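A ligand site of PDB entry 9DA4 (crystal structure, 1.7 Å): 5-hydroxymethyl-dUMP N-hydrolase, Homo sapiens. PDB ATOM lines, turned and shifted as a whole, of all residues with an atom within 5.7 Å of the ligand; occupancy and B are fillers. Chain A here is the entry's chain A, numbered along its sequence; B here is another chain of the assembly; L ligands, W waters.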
ATOM      1  N   TYR A   7     -36.581 -23.996 -24.739  1.00  0.00           N
ATOM      2  CA  TYR A   7     -35.257 -24.494 -24.376  1.00  0.00           C
ATOM      3  C   TYR A   7     -34.988 -24.068 -22.942  1.00  0.00           C
ATOM      4  O   TYR A   7     -34.982 -22.869 -22.665  1.00  0.00           O
ATOM      5  CB  TYR A   7     -34.184 -23.935 -25.321  1.00  0.00           C
ATOM      6  CG  TYR A   7     -32.812 -24.552 -25.199  1.00  0.00           C
ATOM      7  CD1 TYR A   7     -31.963 -24.241 -24.131  1.00  0.00           C
ATOM      8  CD2 TYR A   7     -32.318 -25.408 -26.186  1.00  0.00           C
ATOM      9  CE1 TYR A   7     -30.695 -24.794 -24.023  1.00  0.00           C
ATOM     10  CE2 TYR A   7     -31.052 -25.978 -26.093  1.00  0.00           C
ATOM     11  CZ  TYR A   7     -30.243 -25.672 -25.006  1.00  0.00           C
ATOM     12  OH  TYR A   7     -28.984 -26.205 -24.920  1.00  0.00           O
ATOM     13  N   PHE A   8     -34.786 -25.034 -22.042  1.00  0.00           N
ATOM     14  CA  PHE A   8     -34.484 -24.726 -20.639  1.00  0.00           C
ATOM     15  C   PHE A   8     -33.013 -24.894 -20.339  1.00  0.00           C
ATOM     16  O   PHE A   8     -32.428 -25.946 -20.620  1.00  0.00           O
ATOM     17  CB  PHE A   8     -35.283 -25.606 -19.665  1.00  0.00           C
ATOM     18  CG  PHE A   8     -34.883 -25.367 -18.228  1.00  0.00           C
ATOM     19  CD1 PHE A   8     -35.297 -24.208 -17.569  1.00  0.00           C
ATOM     20  CD2 PHE A   8     -34.016 -26.236 -17.574  1.00  0.00           C
ATOM     21  CE1 PHE A   8     -34.885 -23.947 -16.264  1.00  0.00           C
ATOM     22  CE2 PHE A   8     -33.603 -25.975 -16.269  1.00  0.00           C
ATOM     23  CZ  PHE A   8     -34.050 -24.841 -15.604  1.00  0.00           C
ATOM     24  N   CYS A   9     -32.407 -23.867 -19.723  1.00  0.00           N
ATOM     25  CA  CYS A   9     -31.023 -23.863 -19.295  1.00  0.00           C
ATOM     26  C   CYS A   9     -30.932 -23.904 -17.778  1.00  0.00           C
ATOM     27  O   CYS A   9     -31.631 -23.131 -17.103  1.00  0.00           O
ATOM     28  CB  CYS A   9     -30.295 -22.604 -19.776  1.00  0.00           C
ATOM     29  SG  CYS A   9     -30.553 -22.142 -21.491  1.00  0.00           S
ATOM     30  N   GLY A  10     -30.058 -24.762 -17.249  1.00  0.00           N
ATOM     31  CA  GLY A  10     -29.726 -24.766 -15.836  1.00  0.00           C
ATOM     32  C   GLY A  10     -28.456 -25.547 -15.639  1.00  0.00           C
ATOM     33  O   GLY A  10     -28.183 -26.509 -16.367  1.00  0.00           O
ATOM     34  N   SER A  11     -27.671 -25.159 -14.632  1.00  0.00           N
ATOM     35  CA  SER A  11     -26.350 -25.763 -14.429  1.00  0.00           C
ATOM     36  C   SER A  11     -26.437 -27.289 -14.329  1.00  0.00           C
ATOM     37  O   SER A  11     -27.333 -27.830 -13.673  1.00  0.00           O
ATOM     38  CB  SER A  11     -25.726 -25.177 -13.154  1.00  0.00           C
ATOM     39  OG  SER A  11     -24.541 -25.843 -12.784  1.00  0.00           O
ATOM     40  N   ILE A  12     -25.509 -27.974 -15.007  1.00  0.00           N
ATOM     41  CA  ILE A  12     -25.337 -29.422 -14.868  1.00  0.00           C
ATOM     42  C   ILE A  12     -23.905 -29.720 -14.443  1.00  0.00           C
ATOM     43  O   ILE A  12     -23.657 -30.031 -13.274  1.00  0.00           O
ATOM     44  CB  ILE A  12     -25.695 -30.156 -16.183  1.00  0.00           C
ATOM     45  CG1 ILE A  12     -27.152 -29.870 -16.575  1.00  0.00           C
ATOM     46  CG2 ILE A  12     -25.437 -31.662 -16.035  1.00  0.00           C
ATOM     47  CD1 ILE A  12     -27.565 -30.467 -17.907  1.00  0.00           C
ATOM     48  N   ARG A  13     -22.947 -29.578 -15.352  1.00  0.00           N
ATOM     49  CA  ARG A  13     -21.548 -29.790 -14.934  1.00  0.00           C
ATOM     50  C   ARG A  13     -21.042 -28.662 -14.035  1.00  0.00           C
ATOM     51  O   ARG A  13     -20.106 -28.890 -13.245  1.00  0.00           O
ATOM     52  CB  ARG A  13     -20.647 -29.966 -16.154  1.00  0.00           C
ATOM     53  CG  ARG A  13     -21.083 -31.161 -16.998  1.00  0.00           C
ATOM     54  CD  ARG A  13     -19.984 -31.766 -17.827  1.00  0.00           C
ATOM     55  NE  ARG A  13     -20.515 -32.819 -18.701  1.00  0.00           N
ATOM     56  CZ  ARG A  13     -19.936 -33.258 -19.810  1.00  0.00           C
ATOM     57  NH1 ARG A  13     -18.838 -32.706 -20.276  1.00  0.00           N
ATOM     58  NH2 ARG A  13     -20.487 -34.280 -20.460  1.00  0.00           N
ATOM     59  N   GLY A  14     -21.677 -27.486 -14.082  1.00  0.00           N
ATOM     60  CA  GLY A  14     -21.368 -26.453 -13.107  1.00  0.00           C
ATOM     61  C   GLY A  14     -21.753 -26.836 -11.698  1.00  0.00           C
ATOM     62  O   GLY A  14     -21.250 -26.227 -10.741  1.00  0.00           O
ATOM     63  N   GLY A  15     -22.597 -27.855 -11.548  1.00  0.00           N
ATOM     64  CA  GLY A  15     -23.087 -28.245 -10.241  1.00  0.00           C
ATOM     65  C   GLY A  15     -24.563 -28.502 -10.317  1.00  0.00           C
ATOM     66  O   GLY A  15     -25.289 -27.807 -11.027  1.00  0.00           O
ATOM     67  N   THR A  37     -35.199 -29.712 -24.025  1.00  0.00           N
ATOM     68  CA  THR A  37     -34.076 -30.185 -23.234  1.00  0.00           C
ATOM     69  C   THR A  37     -34.506 -31.087 -22.082  1.00  0.00           C
ATOM     70  O   THR A  37     -33.647 -31.505 -21.299  1.00  0.00           O
ATOM     71  CB  THR A  37     -33.327 -28.981 -22.666  1.00  0.00           C
ATOM     72  OG1 THR A  37     -34.295 -28.094 -22.139  1.00  0.00           O
ATOM     73  CG2 THR A  37     -32.587 -28.260 -23.785  1.00  0.00           C
ATOM     74  N   VAL A  40     -32.792 -34.798 -21.385  1.00  0.00           N
ATOM     75  CA  VAL A  40     -31.338 -34.887 -21.238  1.00  0.00           C
ATOM     76  C   VAL A  40     -30.843 -34.083 -20.045  1.00  0.00           C
ATOM     77  O   VAL A  40     -29.631 -33.955 -19.859  1.00  0.00           O
ATOM     78  CB  VAL A  40     -30.634 -34.481 -22.543  1.00  0.00           C
ATOM     79  CG1 VAL A  40     -30.964 -35.487 -23.638  1.00  0.00           C
ATOM     80  CG2 VAL A  40     -31.105 -33.095 -22.979  1.00  0.00           C
ATOM     81  N   ALA A  41     -31.748 -33.576 -19.209  1.00  0.00           N
ATOM     82  CA  ALA A  41     -31.362 -32.724 -18.078  1.00  0.00           C
ATOM     83  C   ALA A  41     -30.745 -33.521 -16.919  1.00  0.00           C
ATOM     84  O   ALA A  41     -29.947 -32.976 -16.149  1.00  0.00           O
ATOM     85  CB  ALA A  41     -32.590 -31.972 -17.579  1.00  0.00           C
ATOM     86  N   ALA A  42     -31.100 -34.804 -16.773  1.00  0.00           N
ATOM     87  CA  ALA A  42     -30.717 -35.563 -15.593  1.00  0.00           C
ATOM     88  C   ALA A  42     -29.274 -36.065 -15.651  1.00  0.00           C
ATOM     89  O   ALA A  42     -28.684 -36.335 -14.591  1.00  0.00           O
ATOM     90  CB  ALA A  42     -31.666 -36.739 -15.388  1.00  0.00           C
ATOM     91  N   ALA A  43     -28.712 -36.250 -16.851  1.00  0.00           N
ATOM     92  CA  ALA A  43     -27.323 -36.662 -17.030  1.00  0.00           C
ATOM     93  C   ALA A  43     -27.010 -37.921 -16.229  1.00  0.00           C
ATOM     94  O   ALA A  43     -26.059 -37.989 -15.449  1.00  0.00           O
ATOM     95  CB  ALA A  43     -26.361 -35.531 -16.648  1.00  0.00           C
ATOM     96  N   GLU A  50     -20.375 -39.410 -19.420  1.00  0.00           N
ATOM     97  CA  GLU A  50     -20.643 -38.791 -20.714  1.00  0.00           C
ATOM     98  C   GLU A  50     -19.348 -38.442 -21.426  1.00  0.00           C
ATOM     99  O   GLU A  50     -19.204 -38.660 -22.627  1.00  0.00           O
ATOM    100  CB  GLU A  50     -21.514 -37.538 -20.529  1.00  0.00           C
ATOM    101  CG  GLU A  50     -22.911 -37.838 -20.091  1.00  0.00           C
ATOM    102  CD  GLU A  50     -23.735 -36.576 -19.867  1.00  0.00           C
ATOM    103  OE1 GLU A  50     -23.147 -35.466 -19.854  1.00  0.00           O
ATOM    104  OE2 GLU A  50     -24.978 -36.702 -19.752  1.00  0.00           O
ATOM    105  N   ILE A  59     -23.355 -33.513 -27.858  1.00  0.00           N
ATOM    106  CA  ILE A  59     -24.130 -32.683 -26.920  1.00  0.00           C
ATOM    107  C   ILE A  59     -24.153 -31.240 -27.394  1.00  0.00           C
ATOM    108  O   ILE A  59     -25.218 -30.605 -27.417  1.00  0.00           O
ATOM    109  CB  ILE A  59     -23.581 -32.805 -25.495  1.00  0.00           C
ATOM    110  CG1 ILE A  59     -23.793 -34.219 -24.969  1.00  0.00           C
ATOM    111  CG2 ILE A  59     -24.278 -31.800 -24.574  1.00  0.00           C
ATOM    112  CD1 ILE A  59     -23.025 -34.506 -23.668  1.00  0.00           C
ATOM    113  N   ASP A  63     -27.636 -29.774 -29.036  1.00  0.00           N
ATOM    114  CA  ASP A  63     -28.261 -28.732 -28.244  1.00  0.00           C
ATOM    115  C   ASP A  63     -28.339 -27.414 -29.028  1.00  0.00           C
ATOM    116  O   ASP A  63     -29.280 -26.635 -28.843  1.00  0.00           O
ATOM    117  CB  ASP A  63     -27.515 -28.560 -26.914  1.00  0.00           C
ATOM    118  CG  ASP A  63     -27.940 -29.620 -25.895  1.00  0.00           C
ATOM    119  OD1 ASP A  63     -27.266 -30.672 -25.791  1.00  0.00           O
ATOM    120  OD2 ASP A  63     -29.006 -29.477 -25.253  1.00  0.00           O
ATOM    121  N   PRO A  80     -23.783 -20.588 -10.945  1.00  0.00           N
ATOM    122  CA  PRO A  80     -22.909 -20.253 -12.085  1.00  0.00           C
ATOM    123  C   PRO A  80     -22.568 -21.482 -12.922  1.00  0.00           C
ATOM    124  O   PRO A  80     -22.302 -22.568 -12.397  1.00  0.00           O
ATOM    125  CB  PRO A  80     -21.670 -19.638 -11.428  1.00  0.00           C
ATOM    126  CG  PRO A  80     -22.073 -19.266 -10.055  1.00  0.00           C
ATOM    127  CD  PRO A  80     -23.200 -20.199  -9.655  1.00  0.00           C
ATOM    128  N   SER A  81     -22.560 -21.278 -14.236  1.00  0.00           N
ATOM    129  CA  SER A  81     -22.411 -22.392 -15.184  1.00  0.00           C
ATOM    130  C   SER A  81     -21.889 -21.866 -16.509  1.00  0.00           C
ATOM    131  O   SER A  81     -22.480 -20.956 -17.081  1.00  0.00           O
ATOM    132  CB  SER A  81     -23.741 -23.100 -15.406  1.00  0.00           C
ATOM    133  OG  SER A  81     -23.680 -23.966 -16.545  1.00  0.00           O
ATOM    134  N   LEU A  82     -20.797 -22.473 -17.009  1.00  0.00           N
ATOM    135  CA  LEU A  82     -20.291 -22.106 -18.324  1.00  0.00           C
ATOM    136  C   LEU A  82     -21.293 -22.432 -19.417  1.00  0.00           C
ATOM    137  O   LEU A  82     -21.515 -21.636 -20.342  1.00  0.00           O
ATOM    138  CB  LEU A  82     -18.992 -22.867 -18.585  1.00  0.00           C
ATOM    139  CG  LEU A  82     -17.780 -22.520 -17.706  1.00  0.00           C
ATOM    140  CD1 LEU A  82     -16.690 -23.542 -18.021  1.00  0.00           C
ATOM    141  CD2 LEU A  82     -17.297 -21.100 -17.976  1.00  0.00           C
ATOM    142  N   GLY A  83     -21.914 -23.622 -19.337  1.00  0.00           N
ATOM    143  CA  GLY A  83     -22.830 -24.016 -20.389  1.00  0.00           C
ATOM    144  C   GLY A  83     -24.051 -23.120 -20.464  1.00  0.00           C
ATOM    145  O   GLY A  83     -24.528 -22.800 -21.550  1.00  0.00           O
ATOM    146  N   VAL A  84     -24.625 -22.782 -19.306  1.00  0.00           N
ATOM    147  CA  VAL A  84     -25.780 -21.876 -19.291  1.00  0.00           C
ATOM    148  C   VAL A  84     -25.392 -20.539 -19.909  1.00  0.00           C
ATOM    149  O   VAL A  84     -26.124 -19.991 -20.744  1.00  0.00           O
ATOM    150  CB  VAL A  84     -26.304 -21.702 -17.855  1.00  0.00           C
ATOM    151  CG1 VAL A  84     -27.367 -20.605 -17.807  1.00  0.00           C
ATOM    152  CG2 VAL A  84     -26.864 -23.025 -17.348  1.00  0.00           C
ATOM    153  N   GLU A  87     -25.010 -20.974 -23.673  1.00  0.00           N
ATOM    154  CA  GLU A  87     -26.315 -21.057 -24.324  1.00  0.00           C
ATOM    155  C   GLU A  87     -26.956 -19.678 -24.445  1.00  0.00           C
ATOM    156  O   GLU A  87     -27.526 -19.334 -25.484  1.00  0.00           O
ATOM    157  CB  GLU A  87     -27.199 -22.021 -23.545  1.00  0.00           C
ATOM    158  CG  GLU A  87     -26.742 -23.451 -23.765  1.00  0.00           C
ATOM    159  CD  GLU A  87     -27.254 -24.452 -22.755  1.00  0.00           C
ATOM    160  OE1 GLU A  87     -27.719 -24.050 -21.666  1.00  0.00           O
ATOM    161  OE2 GLU A  87     -27.181 -25.658 -23.049  1.00  0.00           O
ATOM    162  N   SER B 111     -17.667 -28.410 -18.688  1.00  0.00           N
ATOM    163  CA  SER B 111     -18.898 -28.224 -19.458  1.00  0.00           C
ATOM    164  C   SER B 111     -18.825 -28.878 -20.835  1.00  0.00           C
ATOM    165  O   SER B 111     -17.878 -28.623 -21.599  1.00  0.00           O
ATOM    166  CB  SER B 111     -19.164 -26.730 -19.633  1.00  0.00           C
ATOM    167  OG  SER B 111     -20.358 -26.501 -20.362  1.00  0.00           O
ATOM    168  N   ALA B 112     -19.831 -29.673 -21.185  1.00  0.00           N
ATOM    169  CA  ALA B 112     -19.853 -30.234 -22.536  1.00  0.00           C
ATOM    170  C   ALA B 112     -20.105 -29.143 -23.570  1.00  0.00           C
ATOM    171  O   ALA B 112     -19.755 -29.318 -24.745  1.00  0.00           O
ATOM    172  CB  ALA B 112     -20.922 -31.339 -22.629  1.00  0.00           C
ATOM    173  N   MET B 113     -20.665 -28.005 -23.157  1.00  0.00           N
ATOM    174  CA  MET B 113     -20.949 -26.971 -24.148  1.00  0.00           C
ATOM    175  C   MET B 113     -19.679 -26.235 -24.522  1.00  0.00           C
ATOM    176  O   MET B 113     -19.615 -25.626 -25.606  1.00  0.00           O
ATOM    177  CB  MET B 113     -22.007 -26.004 -23.628  1.00  0.00           C
ATOM    178  CG  MET B 113     -23.364 -26.723 -23.464  1.00  0.00           C
ATOM    179  SD  MET B 113     -24.040 -27.472 -24.914  1.00  0.00           S
ATOM    180  CE  MET B 113     -24.689 -26.012 -25.753  1.00  0.00           C
HETATM  181  C1  LIG L   1     -24.067 -32.170 -20.541  1.00  0.00           C
HETATM  182  C2  LIG L   1     -26.014 -31.202 -21.328  1.00  0.00           C
HETATM  183  C3  LIG L   1     -26.721 -32.339 -21.000  1.00  0.00           C
HETATM  184  C4  LIG L   1     -27.575 -26.864 -19.512  1.00  0.00           C
HETATM  185  C5  LIG L   1     -26.321 -26.548 -19.664  1.00  0.00           C
HETATM  186  C6  LIG L   1     -25.500 -26.609 -18.306  1.00  0.00           C
HETATM  187  C7  LIG L   1     -25.701 -27.666 -20.685  1.00  0.00           C
HETATM  188  C8  LIG L   1     -26.724 -28.915 -22.505  1.00  0.00           C
HETATM  189  C9  LIG L   1     -27.973 -27.794 -20.854  1.00  0.00           C
HETATM  190  C10 LIG L   1     -26.020 -33.398 -20.384  1.00  0.00           C
HETATM  191  C11 LIG L   1     -28.180 -30.982 -21.860  1.00  0.00           C
HETATM  192  C12 LIG L   1     -26.968 -30.305 -21.878  1.00  0.00           C
HETATM  193  N1  LIG L   1     -26.876 -27.747 -21.634  1.00  0.00           N
HETATM  194  N2  LIG L   1     -24.722 -33.289 -20.214  1.00  0.00           N
HETATM  195  N3  LIG L   1     -24.693 -31.128 -21.092  1.00  0.00           N
HETATM  196  N4  LIG L   1     -26.724 -34.622 -20.017  1.00  0.00           N
HETATM  197  N5  LIG L   1     -28.012 -32.175 -21.313  1.00  0.00           N
HETATM  198  O1  LIG L   1     -28.434 -25.692 -19.552  1.00  0.00           O
HETATM  199  O2  LIG L   1     -24.156 -26.295 -18.620  1.00  0.00           O
HETATM  200  O3  LIG L   1     -23.340 -26.489 -16.214  1.00  0.00           O
HETATM  201  O4  LIG L   1     -21.669 -26.237 -18.057  1.00  0.00           O
HETATM  202  O5  LIG L   1     -22.954 -28.376 -17.794  1.00  0.00           O
HETATM  203  P1  LIG L   1     -22.962 -26.874 -17.631  1.00  0.00           P
HETATM  204  O   HOH W   1     -20.083 -25.133 -16.121  1.00  0.00           O
HETATM  205  O   HOH W   2     -22.456 -29.262 -20.255  1.00  0.00           O
HETATM  206  O   HOH W   3     -31.004 -30.631 -20.463  1.00  0.00           O
HETATM  207  O   HOH W   4     -22.874 -33.997 -17.484  1.00  0.00           O
HETATM  208  O   HOH W   5     -28.633 -36.809 -20.323  1.00  0.00           O
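N of Gly 10 is in hydrogen-bond range of O1 of the ligand (3.0 Å).
The backbone NH of Gly 14 is in hydrogen-bond range of an oxygen (O3) of the ligand.
The backbone NH of Arg 13 sits at hydrogen-bond distance from an oxygen (O5) of the ligand, 2.7 Å away.
The backbone NH of Gly 83 lies within hydrogen-bond range of an oxygen (O4) of the ligand, at 2.9 Å.
O1 of the ligand sits close to O of Gly 10 (3.3 Å).
O3 of the ligand lies within hydrogen-bond range of OG of Ser 81, 2.6 Å away.
The side-chain hydroxyl (OG) of Ser 111 of chain B lies within hydrogen-bond range of an oxygen (O4) of the ligand (2.7 Å).
OE2 of Glu 87 lies within salt-bridge range of N1 of the ligand (2.5 Å).
The backbone carbonyl oxygen of Val 40 lies within hydrogen-bond range of a nitrogen (N5) of the ligand, at 2.8 Å.
OE1 of Glu 50 lies within hydrogen-bond range of N2 of the ligand, at 2.7 Å.
O3 of the ligand sits at hydrogen-bond distance from N of Ile 12, 2.9 Å away.
The side-chain carboxylate of Asp 63 is in hydrogen-bond range of the side-chain hydroxyl of Tyr 7, at 3.3 Å.
The backbone carbonyl oxygen (O) of Ile 59 sits close to the side-chain carboxylate (OD1) of Asp 63 (2.6 Å).
OG of Ser 11 lies within hydrogen-bond range of O of Gly 15.
OE1 of Glu 87 sits at hydrogen-bond distance from SG of Cys 9, 3.4 Å away.
The side-chain hydroxyl (OG) of Ser 111 of chain B is in hydrogen-bond range of the backbone NH (N) of Gly 83, 3.4 Å away.
The backbone NH of Val 84 sits at hydrogen-bond distance from the side-chain hydroxyl of Ser 81, at 3.1 Å.
The side-chain hydroxyl of Ser 81 is in hydrogen-bond range of the backbone NH of Gly 83 (3.3 Å).
The side-chain hydroxyl (OH) of Tyr 7 sits at hydrogen-bond distance from the side-chain carboxylate (OE2) of Glu 87 (2.7 Å).
Merely in contact with the ligand: Cys 9 (3.2 Å), Ser 11 (3.6 Å), Ala 43 (3.5 Å), Ile 59 (3.6 Å), Asp 63 (3.6 Å), Val 84 (3.6 Å), Ala 112 of chain B (3.9 Å) and Met 113 of chain B (3.8 Å).
Along chain A the residues within 4 Å of the ligand span positions 9 to 87.
Water W2 lies within hydrogen-bond range of an oxygen (O5) of the ligand (2.7 Å), the backbone NH (N) of Ala 112 of chain B (2.8 Å) and the side-chain hydroxyl (OG) of Ser 111 of chain B (3.5 Å).
Water W1 lies within hydrogen-bond range of O4 of the ligand (2.7 Å), N of Leu 82 (2.9 Å) and N of Gly 14 (3.5 Å).
Water W5 bridges N4 of the ligand and O of Val 40.
Water W3 lies within hydrogen-bond range of O of Thr 37 (2.9 Å), N of Ala 41 (3.3 Å) and N5 of the ligand (3.5 Å).
Water W4 lies within hydrogen-bond range of the side-chain carboxylate of Glu 50, the guanidinium group of Arg 13 and a nitrogen (N2) of the ligand.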
